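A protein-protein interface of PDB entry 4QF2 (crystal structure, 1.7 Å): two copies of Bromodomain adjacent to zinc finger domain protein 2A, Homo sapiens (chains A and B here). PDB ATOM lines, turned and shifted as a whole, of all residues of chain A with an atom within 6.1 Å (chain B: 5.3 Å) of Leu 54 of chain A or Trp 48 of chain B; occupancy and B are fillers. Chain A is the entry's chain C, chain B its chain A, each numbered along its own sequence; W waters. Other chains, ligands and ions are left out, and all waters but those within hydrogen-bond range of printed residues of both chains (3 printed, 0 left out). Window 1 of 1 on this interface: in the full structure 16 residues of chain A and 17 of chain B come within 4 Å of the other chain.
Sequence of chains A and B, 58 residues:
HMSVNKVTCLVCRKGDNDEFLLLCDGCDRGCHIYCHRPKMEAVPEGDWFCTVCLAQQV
NE2 of Gln 57 of chain A is in hydrogen-bond range of O of Asp 47 of chain B (2.6 Å). The backbone carbonyl oxygen of Glu 45 of chain B lies within hydrogen-bond range of the side-chain amide nitrogen of Gln 57 of chain A (3.0 Å).
The side-chain carboxylate (OD2) of Asp 25 of chain B sits at hydrogen-bond distance from the backbone NH (N) of Trp 48 of chain B (3.0 Å). N of Leu 22 of chain B lies within hydrogen-bond range of O of Cys 31 of chain B, 2.8 Å away.
Among the printed residues, pairs that only touch across the chains: Leu 54 of chain A with Pro 44 of chain B, Gln 57 of chain A with Gly 46 of chain B, Thr 51 of chain A with His 36 of chain B, Thr 51 of chain A with Met 40 of chain B, Leu 54 of chain A with Trp 48 of chain B, Pro 38 of chain A with Cys 31 of chain B and Pro 38 of chain A with His 36 of chain B.
Of the printed residues of chain B, Pro 38 of chain A touches Cys 31 and His 36. Of the printed residues of chain B, Leu 54 of chain A touches Pro 44 (3.5 Å) and Trp 48 (3.9 Å). Printed residues of chain A within 4 Å of His 36 of chain B: Pro 38 (3.96 Å) and Thr 51 (3.7 Å). Of the printed residues of chain A, Pro 44 of chain B touches Leu 54. Printed residues of chain A within 4 Å of Gly 46 of chain B: Gln 57. The nearest residue of chain A that does not touch Trp 48 of chain B is Gln 57 of chain A (4.5 Å).
Hydrophobic or aromatic side chains of chain A within 4 Å of the printed part of chain B: Pro 38 and Leu 54. Of the 18 printed residues of chain B, 8 touch a printed residue of chain A. Hydrophobic or aromatic side chains of chain B within 4 Å of the printed part of chain A: His 36, Met 40, Pro 44 and Trp 48. Along chain B the printed residues that touch a printed residue of chain A span positions 31 to 48.
2 positions are printed for both chains. Of the 9 pairs that touch across the chains among the printed residues, none has its exchanged pair printed and touching as well.
Water W1 lies within hydrogen-bond range of the backbone carbonyl oxygen (O) of Leu 54 of chain A, the backbone NH (N) of Glu 45 of chain B and the backbone carbonyl oxygen (O) of Ala 55 of chain A. Water W3 lies within hydrogen-bond range of the backbone carbonyl oxygen (O) of Asp 47 of chain B and the side-chain amide oxygen (OE1) of Gln 57 of chain A. Water W2 lies within hydrogen-bond range of O of Gln 57 of chain A (2.8 Å) and N of Gly 46 of chain B (3.3 Å).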
ATOM      1  N   PRO A  38       8.049  17.746 -14.084  1.00  0.00           N
ATOM      2  CA  PRO A  38       6.852  16.939 -14.112  1.00  0.00           C
ATOM      3  C   PRO A  38       5.566  17.697 -14.332  1.00  0.00           C
ATOM      4  O   PRO A  38       5.476  18.882 -14.134  1.00  0.00           O
ATOM      5  CB  PRO A  38       6.806  16.305 -12.722  1.00  0.00           C
ATOM      6  CG  PRO A  38       8.173  16.414 -12.186  1.00  0.00           C
ATOM      7  CD  PRO A  38       8.732  17.674 -12.773  1.00  0.00           C
ATOM      8  N   PHE A  49       9.180  28.153  -7.432  1.00  0.00           N
ATOM      9  CA  PHE A  49      10.473  28.762  -7.764  1.00  0.00           C
ATOM     10  C   PHE A  49      10.949  28.149  -9.039  1.00  0.00           C
ATOM     11  O   PHE A  49      10.830  26.942  -9.275  1.00  0.00           O
ATOM     12  CB  PHE A  49      11.502  28.580  -6.646  1.00  0.00           C
ATOM     13  CG  PHE A  49      11.229  29.437  -5.451  1.00  0.00           C
ATOM     14  CD1 PHE A  49      11.595  30.775  -5.426  1.00  0.00           C
ATOM     15  CD2 PHE A  49      10.538  28.922  -4.370  1.00  0.00           C
ATOM     16  CE1 PHE A  49      11.323  31.583  -4.343  1.00  0.00           C
ATOM     17  CE2 PHE A  49      10.266  29.723  -3.289  1.00  0.00           C
ATOM     18  CZ  PHE A  49      10.649  31.052  -3.267  1.00  0.00           C
ATOM     19  N   CYS A  50      11.443  29.000  -9.918  1.00  0.00           N
ATOM     20  CA  CYS A  50      11.921  28.538 -11.169  1.00  0.00           C
ATOM     21  C   CYS A  50      13.284  27.882 -10.911  1.00  0.00           C
ATOM     22  O   CYS A  50      13.852  27.997  -9.839  1.00  0.00           O
ATOM     23  CB  CYS A  50      12.068  29.737 -12.092  1.00  0.00           C
ATOM     24  SG  CYS A  50      13.522  30.792 -11.880  1.00  0.00           S
ATOM     25  N   THR A  51      13.825  27.251 -11.928  1.00  0.00           N
ATOM     26  CA  THR A  51      15.069  26.488 -11.775  1.00  0.00           C
ATOM     27  C   THR A  51      16.271  27.404 -11.566  1.00  0.00           C
ATOM     28  O   THR A  51      17.274  27.014 -10.986  1.00  0.00           O
ATOM     29  CB  THR A  51      15.303  25.569 -12.978  1.00  0.00           C
ATOM     30  OG1 THR A  51      15.107  26.311 -14.178  1.00  0.00           O
ATOM     31  CG2 THR A  51      14.339  24.380 -12.971  1.00  0.00           C
ATOM     32  N   VAL A  52      16.197  28.633 -12.055  1.00  0.00           N
ATOM     33  CA  VAL A  52      17.298  29.583 -11.828  1.00  0.00           C
ATOM     34  C   VAL A  52      17.352  29.956 -10.359  1.00  0.00           C
ATOM     35  O   VAL A  52      18.432  29.904  -9.741  1.00  0.00           O
ATOM     36  CB  VAL A  52      17.123  30.847 -12.671  1.00  0.00           C
ATOM     37  CG1 VAL A  52      18.264  31.825 -12.411  1.00  0.00           C
ATOM     38  CG2 VAL A  52      17.010  30.475 -14.128  1.00  0.00           C
ATOM     39  N   CYS A  53      16.191  30.288  -9.806  1.00  0.00           N
ATOM     40  CA  CYS A  53      16.072  30.582  -8.356  1.00  0.00           C
ATOM     41  C   CYS A  53      16.422  29.364  -7.480  1.00  0.00           C
ATOM     42  O   CYS A  53      17.106  29.504  -6.470  1.00  0.00           O
ATOM     43  CB  CYS A  53      14.688  31.084  -8.056  1.00  0.00           C
ATOM     44  SG  CYS A  53      14.437  32.787  -8.651  1.00  0.00           S
ATOM     45  N   LEU A  54      16.010  28.170  -7.892  1.00  0.00           N
ATOM     46  CA  LEU A  54      16.393  26.946  -7.152  1.00  0.00           C
ATOM     47  C   LEU A  54      17.899  26.753  -7.148  1.00  0.00           C
ATOM     48  O   LEU A  54      18.458  26.216  -6.176  1.00  0.00           O
ATOM     49  CB  LEU A  54      15.729  25.694  -7.727  1.00  0.00           C
ATOM     50  CG  LEU A  54      14.218  25.479  -7.646  1.00  0.00           C
ATOM     51  CD1 LEU A  54      13.779  24.309  -8.524  1.00  0.00           C
ATOM     52  CD2 LEU A  54      13.777  25.238  -6.212  1.00  0.00           C
ATOM     53  N   ALA A  55      18.569  27.150  -8.234  1.00  0.00           N
ATOM     54  CA  ALA A  55      20.016  26.991  -8.380  1.00  0.00           C
ATOM     55  C   ALA A  55      20.776  27.951  -7.445  1.00  0.00           C
ATOM     56  O   ALA A  55      21.935  27.712  -7.118  1.00  0.00           O
ATOM     57  CB  ALA A  55      20.444  27.207  -9.813  1.00  0.00           C
ATOM     58  N   GLN A  56      20.127  29.022  -7.010  1.00  0.00           N
ATOM     59  CA  GLN A  56      20.756  29.938  -6.038  1.00  0.00           C
ATOM     60  C   GLN A  56      20.617  29.528  -4.568  1.00  0.00           C
ATOM     61  O   GLN A  56      21.508  29.808  -3.776  1.00  0.00           O
ATOM     62  CB  GLN A  56      20.252  31.355  -6.279  1.00  0.00           C
ATOM     63  CG  GLN A  56      20.758  31.894  -7.601  1.00  0.00           C
ATOM     64  CD  GLN A  56      20.002  33.122  -8.051  1.00  0.00           C
ATOM     65  OE1 GLN A  56      19.452  33.864  -7.231  1.00  0.00           O
ATOM     66  NE2 GLN A  56      19.972  33.349  -9.354  1.00  0.00           N
ATOM     67  N   GLN A  57      19.530  28.854  -4.202  1.00  0.00           N
ATOM     68  CA  GLN A  57      19.350  28.380  -2.823  1.00  0.00           C
ATOM     69  C   GLN A  57      20.404  27.321  -2.467  1.00  0.00           C
ATOM     70  O   GLN A  57      20.887  27.270  -1.334  1.00  0.00           O
ATOM     71  CB  GLN A  57      17.935  27.806  -2.610  1.00  0.00           C
ATOM     72  CG  GLN A  57      17.715  26.473  -3.312  1.00  0.00           C
ATOM     73  CD  GLN A  57      16.306  25.908  -3.168  1.00  0.00           C
ATOM     74  OE1 GLN A  57      15.305  26.635  -3.230  1.00  0.00           O
ATOM     75  NE2 GLN A  57      16.223  24.592  -3.003  1.00  0.00           N
ATOM     76  N   LEU B  10       9.573  10.787 -11.970  1.00  0.00           N
ATOM     77  CA  LEU B  10       8.166  11.048 -12.304  1.00  0.00           C
ATOM     78  C   LEU B  10       7.864  11.209 -13.789  1.00  0.00           C
ATOM     79  O   LEU B  10       6.764  10.883 -14.223  1.00  0.00           O
ATOM     80  CB  LEU B  10       7.657  12.290 -11.590  1.00  0.00           C
ATOM     81  CG  LEU B  10       7.328  12.176 -10.128  1.00  0.00           C
ATOM     82  CD1 LEU B  10       7.048  13.575  -9.568  1.00  0.00           C
ATOM     83  CD2 LEU B  10       6.128  11.260  -9.897  1.00  0.00           C
ATOM     84  N   LEU B  22      16.831  14.116  -8.694  1.00  0.00           N
ATOM     85  CA  LEU B  22      16.364  15.019  -7.633  1.00  0.00           C
ATOM     86  C   LEU B  22      15.447  14.225  -6.756  1.00  0.00           C
ATOM     87  O   LEU B  22      14.648  13.416  -7.252  1.00  0.00           O
ATOM     88  CB  LEU B  22      15.544  16.164  -8.165  1.00  0.00           C
ATOM     89  CG  LEU B  22      16.068  17.135  -9.177  1.00  0.00           C
ATOM     90  CD1 LEU B  22      14.893  17.806  -9.886  1.00  0.00           C
ATOM     91  CD2 LEU B  22      16.962  18.122  -8.452  1.00  0.00           C
ATOM     92  N   LEU B  23      15.538  14.443  -5.434  1.00  0.00           N
ATOM     93  CA  LEU B  23      14.660  13.742  -4.501  1.00  0.00           C
ATOM     94  C   LEU B  23      13.792  14.755  -3.767  1.00  0.00           C
ATOM     95  O   LEU B  23      14.304  15.777  -3.271  1.00  0.00           O
ATOM     96  CB  LEU B  23      15.493  12.950  -3.479  1.00  0.00           C
ATOM     97  CG  LEU B  23      16.468  11.964  -4.114  1.00  0.00           C
ATOM     98  CD1 LEU B  23      17.393  11.332  -3.075  1.00  0.00           C
ATOM     99  CD2 LEU B  23      15.656  10.910  -4.850  1.00  0.00           C
ATOM    100  N   CYS B  24      12.479  14.503  -3.763  1.00  0.00           N
ATOM    101  CA  CYS B  24      11.511  15.435  -3.184  1.00  0.00           C
ATOM    102  C   CYS B  24      11.670  15.426  -1.686  1.00  0.00           C
ATOM    103  O   CYS B  24      11.772  14.365  -1.070  1.00  0.00           O
ATOM    104  CB  CYS B  24      10.055  15.044  -3.520  1.00  0.00           C
ATOM    105  SG  CYS B  24       8.804  16.203  -2.913  1.00  0.00           S
ATOM    106  N   ASP B  25      11.656  16.615  -1.112  1.00  0.00           N
ATOM    107  CA  ASP B  25      11.730  16.765   0.345  1.00  0.00           C
ATOM    108  C   ASP B  25      10.384  16.586   1.066  1.00  0.00           C
ATOM    109  O   ASP B  25      10.336  16.500   2.311  1.00  0.00           O
ATOM    110  CB  ASP B  25      12.368  18.093   0.628  1.00  0.00           C
ATOM    111  CG  ASP B  25      13.850  18.088   0.293  1.00  0.00           C
ATOM    112  OD1 ASP B  25      14.573  17.195   0.791  1.00  0.00           O
ATOM    113  OD2 ASP B  25      14.304  18.943  -0.488  1.00  0.00           O
ATOM    114  N   GLY B  26       9.307  16.480   0.300  1.00  0.00           N
ATOM    115  CA  GLY B  26       7.966  16.261   0.820  1.00  0.00           C
ATOM    116  C   GLY B  26       7.393  14.845   0.724  1.00  0.00           C
ATOM    117  O   GLY B  26       6.350  14.564   1.331  1.00  0.00           O
ATOM    118  N   ARG B  29       8.976  10.819  -3.987  1.00  0.00           N
ATOM    119  CA  ARG B  29       9.027  10.937  -5.446  1.00  0.00           C
ATOM    120  C   ARG B  29      10.338  11.555  -5.902  1.00  0.00           C
ATOM    121  O   ARG B  29      11.088  12.179  -5.122  1.00  0.00           O
ATOM    122  CB  ARG B  29       7.842  11.739  -5.993  1.00  0.00           C
ATOM    123  CG  ARG B  29       6.504  11.075  -5.792  1.00  0.00           C
ATOM    124  CD  ARG B  29       5.361  11.926  -6.274  1.00  0.00           C
ATOM    125  NE  ARG B  29       4.097  11.239  -6.029  1.00  0.00           N
ATOM    126  CZ  ARG B  29       3.466  11.251  -4.864  1.00  0.00           C
ATOM    127  NH1 ARG B  29       3.971  11.916  -3.828  1.00  0.00           N
ATOM    128  NH2 ARG B  29       2.324  10.595  -4.726  1.00  0.00           N
ATOM    129  N   GLY B  30      10.658  11.323  -7.171  1.00  0.00           N
ATOM    130  CA  GLY B  30      11.914  11.855  -7.731  1.00  0.00           C
ATOM    131  C   GLY B  30      11.788  12.341  -9.145  1.00  0.00           C
ATOM    132  O   GLY B  30      10.748  12.185  -9.782  1.00  0.00           O
ATOM    133  N   CYS B  31      12.868  12.962  -9.645  1.00  0.00           N
ATOM    134  CA  CYS B  31      12.891  13.439 -11.036  1.00  0.00           C
ATOM    135  C   CYS B  31      14.336  13.574 -11.502  1.00  0.00           C
ATOM    136  O   CYS B  31      15.095  14.214 -10.830  1.00  0.00           O
ATOM    137  CB  CYS B  31      12.212  14.809 -11.164  1.00  0.00           C
ATOM    138  SG  CYS B  31      11.949  15.391 -12.850  1.00  0.00           S
ATOM    139  N   HIS B  36      13.550  17.259 -16.163  1.00  0.00           N
ATOM    140  CA  HIS B  36      12.847  18.438 -15.665  1.00  0.00           C
ATOM    141  C   HIS B  36      12.738  19.497 -16.756  1.00  0.00           C
ATOM    142  O   HIS B  36      13.648  19.709 -17.568  1.00  0.00           O
ATOM    143  CB  HIS B  36      13.575  18.973 -14.453  1.00  0.00           C
ATOM    144  CG  HIS B  36      12.763  19.881 -13.595  1.00  0.00           C
ATOM    145  ND1 HIS B  36      12.517  21.202 -13.937  1.00  0.00           N
ATOM    146  CD2 HIS B  36      12.138  19.663 -12.429  1.00  0.00           C
ATOM    147  CE1 HIS B  36      11.775  21.753 -12.991  1.00  0.00           C
ATOM    148  NE2 HIS B  36      11.551  20.860 -12.053  1.00  0.00           N
ATOM    149  N   MET B  40      17.050  22.216 -15.726  1.00  0.00           N
ATOM    150  CA  MET B  40      17.731  22.091 -14.434  1.00  0.00           C
ATOM    151  C   MET B  40      19.091  21.478 -14.714  1.00  0.00           C
ATOM    152  O   MET B  40      19.171  20.301 -15.066  1.00  0.00           O
ATOM    153  CB  MET B  40      16.886  21.334 -13.445  1.00  0.00           C
ATOM    154  CG  MET B  40      17.550  21.156 -12.123  1.00  0.00           C
ATOM    155  SD  MET B  40      16.456  20.201 -11.048  1.00  0.00           S
ATOM    156  CE  MET B  40      15.065  21.297 -10.870  1.00  0.00           C
ATOM    157  N   PRO B  44      19.884  20.839  -7.069  1.00  0.00           N
ATOM    158  CA  PRO B  44      20.071  21.989  -6.171  1.00  0.00           C
ATOM    159  C   PRO B  44      20.360  21.585  -4.736  1.00  0.00           C
ATOM    160  O   PRO B  44      20.093  20.447  -4.317  1.00  0.00           O
ATOM    161  CB  PRO B  44      18.725  22.724  -6.230  1.00  0.00           C
ATOM    162  CG  PRO B  44      17.733  21.700  -6.622  1.00  0.00           C
ATOM    163  CD  PRO B  44      18.465  20.673  -7.458  1.00  0.00           C
ATOM    164  N   GLU B  45      20.877  22.538  -3.991  1.00  0.00           N
ATOM    165  CA  GLU B  45      21.005  22.372  -2.550  1.00  0.00           C
ATOM    166  C   GLU B  45      19.799  23.010  -1.897  1.00  0.00           C
ATOM    167  O   GLU B  45      19.012  23.683  -2.550  1.00  0.00           O
ATOM    168  CB  GLU B  45      22.298  22.982  -2.094  1.00  0.00           C
ATOM    169  CG  GLU B  45      23.471  22.241  -2.703  1.00  0.00           C
ATOM    170  CD  GLU B  45      24.741  22.380  -1.906  1.00  0.00           C
ATOM    171  OE1 GLU B  45      24.701  22.171  -0.673  1.00  0.00           O
ATOM    172  OE2 GLU B  45      25.782  22.677  -2.523  1.00  0.00           O
ATOM    173  N   GLY B  46      19.617  22.753  -0.615  1.00  0.00           N
ATOM    174  CA  GLY B  46      18.352  23.084   0.008  1.00  0.00           C
ATOM    175  C   GLY B  46      17.277  22.227  -0.634  1.00  0.00           C
ATOM    176  O   GLY B  46      17.545  21.109  -1.086  1.00  0.00           O
ATOM    177  N   ASP B  47      16.062  22.747  -0.708  1.00  0.00           N
ATOM    178  CA  ASP B  47      14.926  21.870  -0.956  1.00  0.00           C
ATOM    179  C   ASP B  47      14.275  21.943  -2.316  1.00  0.00           C
ATOM    180  O   ASP B  47      14.120  23.003  -2.898  1.00  0.00           O
ATOM    181  CB  ASP B  47      13.868  22.093   0.116  1.00  0.00           C
ATOM    182  CG  ASP B  47      14.400  21.838   1.517  1.00  0.00           C
ATOM    183  OD1 ASP B  47      15.306  20.982   1.691  1.00  0.00           O
ATOM    184  OD2 ASP B  47      13.904  22.505   2.439  1.00  0.00           O
ATOM    185  N   TRP B  48      13.840  20.781  -2.787  1.00  0.00           N
ATOM    186  CA  TRP B  48      13.097  20.669  -4.030  1.00  0.00           C
ATOM    187  C   TRP B  48      11.792  19.911  -3.750  1.00  0.00           C
ATOM    188  O   TRP B  48      11.776  18.911  -3.018  1.00  0.00           O
ATOM    189  CB  TRP B  48      13.923  20.008  -5.137  1.00  0.00           C
ATOM    190  CG  TRP B  48      13.129  19.800  -6.367  1.00  0.00           C
ATOM    191  CD1 TRP B  48      12.818  20.731  -7.313  1.00  0.00           C
ATOM    192  CD2 TRP B  48      12.488  18.595  -6.774  1.00  0.00           C
ATOM    193  NE1 TRP B  48      12.032  20.181  -8.271  1.00  0.00           N
ATOM    194  CE2 TRP B  48      11.824  18.865  -7.973  1.00  0.00           C
ATOM    195  CE3 TRP B  48      12.411  17.299  -6.234  1.00  0.00           C
ATOM    196  CZ2 TRP B  48      11.089  17.910  -8.636  1.00  0.00           C
ATOM    197  CZ3 TRP B  48      11.701  16.340  -6.923  1.00  0.00           C
ATOM    198  CH2 TRP B  48      11.057  16.657  -8.111  1.00  0.00           C
ATOM    199  N   PHE B  49      10.687  20.433  -4.287  1.00  0.00           N
ATOM    200  CA  PHE B  49       9.400  19.765  -4.162  1.00  0.00           C
ATOM    201  C   PHE B  49       8.865  19.390  -5.510  1.00  0.00           C
ATOM    202  O   PHE B  49       8.916  20.165  -6.491  1.00  0.00           O
ATOM    203  CB  PHE B  49       8.366  20.574  -3.381  1.00  0.00           C
ATOM    204  CG  PHE B  49       8.776  20.838  -1.967  1.00  0.00           C
ATOM    205  CD1 PHE B  49       8.577  19.884  -0.992  1.00  0.00           C
ATOM    206  CD2 PHE B  49       9.443  22.005  -1.644  1.00  0.00           C
ATOM    207  CE1 PHE B  49       8.972  20.116   0.319  1.00  0.00           C
ATOM    208  CE2 PHE B  49       9.850  22.244  -0.347  1.00  0.00           C
ATOM    209  CZ  PHE B  49       9.632  21.280   0.632  1.00  0.00           C
ATOM    210  N   CYS B  50       8.397  18.157  -5.560  1.00  0.00           N
ATOM    211  CA  CYS B  50       7.728  17.641  -6.700  1.00  0.00           C
ATOM    212  C   CYS B  50       6.361  18.292  -6.835  1.00  0.00           C
ATOM    213  O   CYS B  50       5.859  18.954  -5.936  1.00  0.00           O
ATOM    214  CB  CYS B  50       7.559  16.143  -6.600  1.00  0.00           C
ATOM    215  SG  CYS B  50       6.199  15.585  -5.531  1.00  0.00           S
HETATM  216  O   HOH W   1      20.774  25.234  -5.155  1.00  0.00           O
HETATM  217  O   HOH W   2      20.832  25.486   0.787  1.00  0.00           O
HETATM  218  O   HOH W   3      12.300  25.013  -3.164  1.00  0.00           O
